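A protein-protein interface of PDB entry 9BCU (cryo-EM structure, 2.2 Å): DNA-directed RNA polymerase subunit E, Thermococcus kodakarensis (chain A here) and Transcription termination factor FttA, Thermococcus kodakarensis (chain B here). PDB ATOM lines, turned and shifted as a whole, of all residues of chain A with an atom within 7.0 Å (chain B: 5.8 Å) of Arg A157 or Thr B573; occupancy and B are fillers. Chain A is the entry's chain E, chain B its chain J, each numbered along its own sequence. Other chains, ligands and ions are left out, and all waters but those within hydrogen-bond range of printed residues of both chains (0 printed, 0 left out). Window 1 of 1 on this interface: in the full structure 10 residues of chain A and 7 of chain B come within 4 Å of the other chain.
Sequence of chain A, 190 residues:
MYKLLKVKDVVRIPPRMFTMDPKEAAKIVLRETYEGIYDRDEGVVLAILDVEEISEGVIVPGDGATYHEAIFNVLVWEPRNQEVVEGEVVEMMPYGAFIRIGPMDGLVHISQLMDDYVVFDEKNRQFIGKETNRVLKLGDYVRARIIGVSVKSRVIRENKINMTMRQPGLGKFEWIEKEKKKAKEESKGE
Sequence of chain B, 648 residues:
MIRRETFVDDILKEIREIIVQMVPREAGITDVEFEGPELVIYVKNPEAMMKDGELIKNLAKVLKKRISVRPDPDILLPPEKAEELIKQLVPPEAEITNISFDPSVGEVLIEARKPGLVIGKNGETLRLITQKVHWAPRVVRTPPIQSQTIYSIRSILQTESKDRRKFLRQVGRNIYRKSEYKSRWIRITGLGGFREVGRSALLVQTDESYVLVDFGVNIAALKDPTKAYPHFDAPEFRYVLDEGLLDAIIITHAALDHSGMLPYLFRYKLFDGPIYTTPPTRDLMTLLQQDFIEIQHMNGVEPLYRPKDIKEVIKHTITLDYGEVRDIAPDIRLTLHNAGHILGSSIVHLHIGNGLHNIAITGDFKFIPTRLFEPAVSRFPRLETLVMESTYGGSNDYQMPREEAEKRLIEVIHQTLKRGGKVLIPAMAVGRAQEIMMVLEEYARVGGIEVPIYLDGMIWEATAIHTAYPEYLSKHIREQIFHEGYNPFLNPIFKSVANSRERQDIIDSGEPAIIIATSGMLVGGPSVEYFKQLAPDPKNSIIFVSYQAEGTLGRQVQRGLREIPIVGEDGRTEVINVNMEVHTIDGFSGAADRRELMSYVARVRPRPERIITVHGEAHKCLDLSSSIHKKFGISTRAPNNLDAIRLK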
ATOM      1  N   GLY A  36      -1.314  18.828  20.255  1.00  0.00           N
ATOM      2  CA  GLY A  36      -1.853  18.640  21.584  1.00  0.00           C
ATOM      3  C   GLY A  36      -1.697  19.797  22.545  1.00  0.00           C
ATOM      4  O   GLY A  36      -2.016  19.636  23.729  1.00  0.00           O
ATOM      5  N   TYR A  38      -1.945  24.340  23.167  1.00  0.00           N
ATOM      6  CA  TYR A  38      -2.627  25.565  22.771  1.00  0.00           C
ATOM      7  C   TYR A  38      -1.594  26.634  22.446  1.00  0.00           C
ATOM      8  O   TYR A  38      -0.702  26.910  23.254  1.00  0.00           O
ATOM      9  CB  TYR A  38      -3.562  26.051  23.882  1.00  0.00           C
ATOM     10  CG  TYR A  38      -4.565  27.098  23.446  1.00  0.00           C
ATOM     11  CD1 TYR A  38      -4.205  28.436  23.341  1.00  0.00           C
ATOM     12  CD2 TYR A  38      -5.876  26.751  23.149  1.00  0.00           C
ATOM     13  CE1 TYR A  38      -5.117  29.394  22.945  1.00  0.00           C
ATOM     14  CE2 TYR A  38      -6.796  27.704  22.755  1.00  0.00           C
ATOM     15  CZ  TYR A  38      -6.411  29.023  22.655  1.00  0.00           C
ATOM     16  OH  TYR A  38      -7.323  29.975  22.261  1.00  0.00           O
ATOM     17  N   PRO A 103     -12.734  21.454  19.680  1.00  0.00           N
ATOM     18  CA  PRO A 103     -11.705  20.924  20.588  1.00  0.00           C
ATOM     19  C   PRO A 103     -11.852  21.412  22.019  1.00  0.00           C
ATOM     20  O   PRO A 103     -11.292  20.786  22.928  1.00  0.00           O
ATOM     21  CB  PRO A 103     -10.394  21.414  19.960  1.00  0.00           C
ATOM     22  CG  PRO A 103     -10.776  22.629  19.197  1.00  0.00           C
ATOM     23  CD  PRO A 103     -12.186  22.425  18.717  1.00  0.00           C
ATOM     24  N   MET A 104     -12.582  22.501  22.247  1.00  0.00           N
ATOM     25  CA  MET A 104     -12.799  23.040  23.581  1.00  0.00           C
ATOM     26  C   MET A 104     -14.295  23.148  23.844  1.00  0.00           C
ATOM     27  O   MET A 104     -15.106  23.231  22.918  1.00  0.00           O
ATOM     28  CB  MET A 104     -12.138  24.415  23.751  1.00  0.00           C
ATOM     29  CG  MET A 104     -10.742  24.517  23.161  1.00  0.00           C
ATOM     30  SD  MET A 104      -9.983  26.120  23.476  1.00  0.00           S
ATOM     31  CE  MET A 104     -10.068  26.183  25.263  1.00  0.00           C
ATOM     32  N   ASP A 105     -14.651  23.144  25.124  1.00  0.00           N
ATOM     33  CA  ASP A 105     -16.038  23.230  25.558  1.00  0.00           C
ATOM     34  C   ASP A 105     -16.279  24.570  26.236  1.00  0.00           C
ATOM     35  O   ASP A 105     -15.576  24.926  27.188  1.00  0.00           O
ATOM     36  CB  ASP A 105     -16.384  22.087  26.515  1.00  0.00           C
ATOM     37  CG  ASP A 105     -16.392  20.735  25.830  1.00  0.00           C
ATOM     38  OD1 ASP A 105     -16.142  20.685  24.607  1.00  0.00           O
ATOM     39  OD2 ASP A 105     -16.651  19.722  26.514  1.00  0.00           O
ATOM     40  N   SER A 153      -2.812  30.111  29.651  1.00  0.00           N
ATOM     41  CA  SER A 153      -1.887  28.989  29.694  1.00  0.00           C
ATOM     42  C   SER A 153      -1.888  28.251  28.363  1.00  0.00           C
ATOM     43  O   SER A 153      -2.829  28.345  27.572  1.00  0.00           O
ATOM     44  CB  SER A 153      -2.237  28.018  30.828  1.00  0.00           C
ATOM     45  OG  SER A 153      -2.961  26.903  30.338  1.00  0.00           O
ATOM     46  N   ARG A 154      -0.805  27.508  28.129  1.00  0.00           N
ATOM     47  CA  ARG A 154      -0.660  26.706  26.922  1.00  0.00           C
ATOM     48  C   ARG A 154      -1.426  25.391  26.983  1.00  0.00           C
ATOM     49  O   ARG A 154      -1.481  24.679  25.974  1.00  0.00           O
ATOM     50  CB  ARG A 154       0.821  26.419  26.655  1.00  0.00           C
ATOM     51  CG  ARG A 154       1.481  27.397  25.699  1.00  0.00           C
ATOM     52  CD  ARG A 154       2.992  27.393  25.863  1.00  0.00           C
ATOM     53  NE  ARG A 154       3.584  26.137  25.423  1.00  0.00           N
ATOM     54  CZ  ARG A 154       3.883  25.848  24.163  1.00  0.00           C
ATOM     55  NH1 ARG A 154       3.656  26.709  23.185  1.00  0.00           N
ATOM     56  NH2 ARG A 154       4.422  24.666  23.878  1.00  0.00           N
ATOM     57  N   VAL A 155      -2.002  25.048  28.131  1.00  0.00           N
ATOM     58  CA  VAL A 155      -2.795  23.831  28.256  1.00  0.00           C
ATOM     59  C   VAL A 155      -4.209  24.113  27.767  1.00  0.00           C
ATOM     60  O   VAL A 155      -4.824  25.114  28.151  1.00  0.00           O
ATOM     61  CB  VAL A 155      -2.795  23.328  29.707  1.00  0.00           C
ATOM     62  CG1 VAL A 155      -3.381  21.928  29.783  1.00  0.00           C
ATOM     63  CG2 VAL A 155      -1.384  23.353  30.275  1.00  0.00           C
ATOM     64  N   ILE A 156      -4.723  23.231  26.907  1.00  0.00           N
ATOM     65  CA  ILE A 156      -6.057  23.425  26.345  1.00  0.00           C
ATOM     66  C   ILE A 156      -7.122  23.307  27.429  1.00  0.00           C
ATOM     67  O   ILE A 156      -8.091  24.077  27.449  1.00  0.00           O
ATOM     68  CB  ILE A 156      -6.303  22.425  25.201  1.00  0.00           C
ATOM     69  CG1 ILE A 156      -5.041  22.263  24.353  1.00  0.00           C
ATOM     70  CG2 ILE A 156      -7.472  22.877  24.341  1.00  0.00           C
ATOM     71  CD1 ILE A 156      -5.058  21.041  23.463  1.00  0.00           C
ATOM     72  N   ARG A 157      -6.967  22.343  28.339  1.00  0.00           N
ATOM     73  CA  ARG A 157      -7.969  22.137  29.379  1.00  0.00           C
ATOM     74  C   ARG A 157      -7.992  23.282  30.384  1.00  0.00           C
ATOM     75  O   ARG A 157      -9.051  23.593  30.942  1.00  0.00           O
ATOM     76  CB  ARG A 157      -7.716  20.811  30.095  1.00  0.00           C
ATOM     77  CG  ARG A 157      -7.610  19.615  29.166  1.00  0.00           C
ATOM     78  CD  ARG A 157      -8.975  19.005  28.896  1.00  0.00           C
ATOM     79  NE  ARG A 157      -9.596  18.497  30.113  1.00  0.00           N
ATOM     80  CZ  ARG A 157     -10.883  18.202  30.230  1.00  0.00           C
ATOM     81  NH1 ARG A 157     -11.722  18.355  29.219  1.00  0.00           N
ATOM     82  NH2 ARG A 157     -11.340  17.743  31.391  1.00  0.00           N
ATOM     83  N   GLU A 158      -6.844  23.918  30.631  1.00  0.00           N
ATOM     84  CA  GLU A 158      -6.800  25.007  31.601  1.00  0.00           C
ATOM     85  C   GLU A 158      -7.467  26.268  31.066  1.00  0.00           C
ATOM     86  O   GLU A 158      -7.949  27.092  31.854  1.00  0.00           O
ATOM     87  CB  GLU A 158      -5.354  25.295  32.001  1.00  0.00           C
ATOM     88  CG  GLU A 158      -4.714  24.189  32.826  1.00  0.00           C
ATOM     89  CD  GLU A 158      -3.309  24.534  33.277  1.00  0.00           C
ATOM     90  OE1 GLU A 158      -2.870  25.677  33.037  1.00  0.00           O
ATOM     91  OE2 GLU A 158      -2.644  23.659  33.872  1.00  0.00           O
ATOM     92  N   ASN A 159      -7.503  26.441  29.749  1.00  0.00           N
ATOM     93  CA  ASN A 159      -8.168  27.597  29.164  1.00  0.00           C
ATOM     94  C   ASN A 159      -9.680  27.462  29.292  1.00  0.00           C
ATOM     95  O   ASN A 159     -10.232  26.361  29.211  1.00  0.00           O
ATOM     96  CB  ASN A 159      -7.773  27.752  27.696  1.00  0.00           C
ATOM     97  CG  ASN A 159      -6.308  28.095  27.521  1.00  0.00           C
ATOM     98  OD1 ASN A 159      -5.738  28.854  28.304  1.00  0.00           O
ATOM     99  ND2 ASN A 159      -5.689  27.536  26.487  1.00  0.00           N
ATOM    100  N   LYS A 160     -10.352  28.593  29.492  1.00  0.00           N
ATOM    101  CA  LYS A 160     -11.792  28.625  29.695  1.00  0.00           C
ATOM    102  C   LYS A 160     -12.460  29.447  28.602  1.00  0.00           C
ATOM    103  O   LYS A 160     -11.917  30.452  28.136  1.00  0.00           O
ATOM    104  CB  LYS A 160     -12.146  29.205  31.070  1.00  0.00           C
ATOM    105  CG  LYS A 160     -11.498  28.476  32.235  1.00  0.00           C
ATOM    106  CD  LYS A 160     -12.373  27.337  32.729  1.00  0.00           C
ATOM    107  CE  LYS A 160     -12.457  27.326  34.246  1.00  0.00           C
ATOM    108  NZ  LYS A 160     -11.150  27.659  34.876  1.00  0.00           N
ATOM    109  N   PRO B 565     -11.241  12.998  30.708  1.00  0.00           N
ATOM    110  CA  PRO B 565     -10.062  13.717  30.205  1.00  0.00           C
ATOM    111  C   PRO B 565      -9.387  14.500  31.324  1.00  0.00           C
ATOM    112  O   PRO B 565     -10.028  15.286  32.026  1.00  0.00           O
ATOM    113  CB  PRO B 565     -10.640  14.649  29.136  1.00  0.00           C
ATOM    114  CG  PRO B 565     -12.064  14.862  29.543  1.00  0.00           C
ATOM    115  CD  PRO B 565     -12.502  13.690  30.387  1.00  0.00           C
ATOM    116  N   ILE B 566      -8.083  14.276  31.489  1.00  0.00           N
ATOM    117  CA  ILE B 566      -7.292  14.941  32.513  1.00  0.00           C
ATOM    118  C   ILE B 566      -6.026  15.496  31.876  1.00  0.00           C
ATOM    119  O   ILE B 566      -5.610  15.080  30.793  1.00  0.00           O
ATOM    120  CB  ILE B 566      -6.930  14.001  33.684  1.00  0.00           C
ATOM    121  CG1 ILE B 566      -6.188  12.770  33.163  1.00  0.00           C
ATOM    122  CG2 ILE B 566      -8.177  13.600  34.460  1.00  0.00           C
ATOM    123  CD1 ILE B 566      -4.946  12.428  33.952  1.00  0.00           C
ATOM    124  N   VAL B 567      -5.413  16.449  32.570  1.00  0.00           N
ATOM    125  CA  VAL B 567      -4.165  17.049  32.110  1.00  0.00           C
ATOM    126  C   VAL B 567      -3.013  16.110  32.444  1.00  0.00           C
ATOM    127  O   VAL B 567      -2.845  15.699  33.598  1.00  0.00           O
ATOM    128  CB  VAL B 567      -3.960  18.432  32.746  1.00  0.00           C
ATOM    129  CG1 VAL B 567      -2.571  18.964  32.427  1.00  0.00           C
ATOM    130  CG2 VAL B 567      -5.030  19.399  32.268  1.00  0.00           C
ATOM    131  N   GLY B 568      -2.216  15.771  31.434  1.00  0.00           N
ATOM    132  CA  GLY B 568      -1.096  14.877  31.621  1.00  0.00           C
ATOM    133  C   GLY B 568       0.123  15.576  32.192  1.00  0.00           C
ATOM    134  O   GLY B 568       0.131  16.776  32.464  1.00  0.00           O
ATOM    135  N   GLY B 571       1.708  18.175  29.737  1.00  0.00           N
ATOM    136  CA  GLY B 571       0.869  19.293  29.364  1.00  0.00           C
ATOM    137  C   GLY B 571      -0.195  18.985  28.335  1.00  0.00           C
ATOM    138  O   GLY B 571      -0.902  19.905  27.908  1.00  0.00           O
ATOM    139  N   ARG B 572      -0.332  17.730  27.923  1.00  0.00           N
ATOM    140  CA  ARG B 572      -1.354  17.319  26.973  1.00  0.00           C
ATOM    141  C   ARG B 572      -2.477  16.583  27.692  1.00  0.00           C
ATOM    142  O   ARG B 572      -2.300  16.044  28.787  1.00  0.00           O
ATOM    143  CB  ARG B 572      -0.756  16.427  25.882  1.00  0.00           C
ATOM    144  CG  ARG B 572       0.696  16.729  25.555  1.00  0.00           C
ATOM    145  CD  ARG B 572       0.809  17.683  24.379  1.00  0.00           C
ATOM    146  NE  ARG B 572       2.150  18.242  24.258  1.00  0.00           N
ATOM    147  CZ  ARG B 572       2.970  18.010  23.243  1.00  0.00           C
ATOM    148  NH1 ARG B 572       2.617  17.229  22.234  1.00  0.00           N
ATOM    149  NH2 ARG B 572       4.173  18.576  23.239  1.00  0.00           N
ATOM    150  N   THR B 573      -3.648  16.574  27.059  1.00  0.00           N
ATOM    151  CA  THR B 573      -4.803  15.900  27.634  1.00  0.00           C
ATOM    152  C   THR B 573      -4.590  14.391  27.654  1.00  0.00           C
ATOM    153  O   THR B 573      -4.108  13.801  26.683  1.00  0.00           O
ATOM    154  CB  THR B 573      -6.066  16.240  26.842  1.00  0.00           C
ATOM    155  OG1 THR B 573      -6.080  17.642  26.543  1.00  0.00           O
ATOM    156  CG2 THR B 573      -7.309  15.886  27.643  1.00  0.00           C
ATOM    157  N   GLU B 574      -4.953  13.769  28.771  1.00  0.00           N
ATOM    158  CA  GLU B 574      -4.846  12.329  28.948  1.00  0.00           C
ATOM    159  C   GLU B 574      -6.223  11.753  29.242  1.00  0.00           C
ATOM    160  O   GLU B 574      -7.040  12.386  29.918  1.00  0.00           O
ATOM    161  CB  GLU B 574      -3.877  11.980  30.082  1.00  0.00           C
ATOM    162  CG  GLU B 574      -2.958  10.810  29.775  1.00  0.00           C
ATOM    163  CD  GLU B 574      -2.452  10.122  31.027  1.00  0.00           C
ATOM    164  OE1 GLU B 574      -2.766  10.599  32.137  1.00  0.00           O
ATOM    165  OE2 GLU B 574      -1.738   9.105  30.902  1.00  0.00           O
ATOM    166  N   VAL B 575      -6.475  10.550  28.733  1.00  0.00           N
ATOM    167  CA  VAL B 575      -7.763   9.881  28.876  1.00  0.00           C
ATOM    168  C   VAL B 575      -7.588   8.693  29.811  1.00  0.00           C
ATOM    169  O   VAL B 575      -6.727   7.835  29.581  1.00  0.00           O
ATOM    170  CB  VAL B 575      -8.319   9.431  27.514  1.00  0.00           C
ATOM    171  CG1 VAL B 575      -9.648   8.716  27.694  1.00  0.00           C
ATOM    172  CG2 VAL B 575      -8.471  10.625  26.586  1.00  0.00           C
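O of Pro B565 is in hydrogen-bond range of NH2 of Arg A157 (2.9 Å).
The backbone NH of Val A155 sits at hydrogen-bond distance from the side-chain hydroxyl of Ser A153 (3.0 Å).
The backbone carbonyl oxygen of Val A155 is in hydrogen-bond range of the side-chain amide nitrogen of Asn A159 (3.1 Å).
Among the printed residues, pairs that only touch across the chains: Gly A36 with Arg B572, Val A155 with Val B567, Val A155 with Gly B571, Arg A157 with Val B567 and Arg A157 with Thr B573.
Arg A157 touches just these residues of chain B: Pro B565 (2.9 Å), Val B567 (3.7 Å) and Thr B573 (3.6 Å).
Of the printed residues of chain A, Thr B573 touches Arg A157 (3.6 Å).
Of the printed residues of chain A, Pro B565 touches Arg A157 (2.9 Å).
Printed residues of chain B within 4 Å of Gly A36: Arg B572 (3.5 Å).
Pro A103 touches none of the printed residues of chain B.
Ile B566 touches none of the printed residues of chain A.
The nearest residue of chain A that does not touch Thr B573 is Ile A156 (4.7 Å).
Of the 9 printed residues of chain B, 5 touch a printed residue of chain A.
Among the printed residues, no Asp or Glu carboxylate lies within 4 Å of a Lys or Arg side-chain nitrogen of the other chain.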
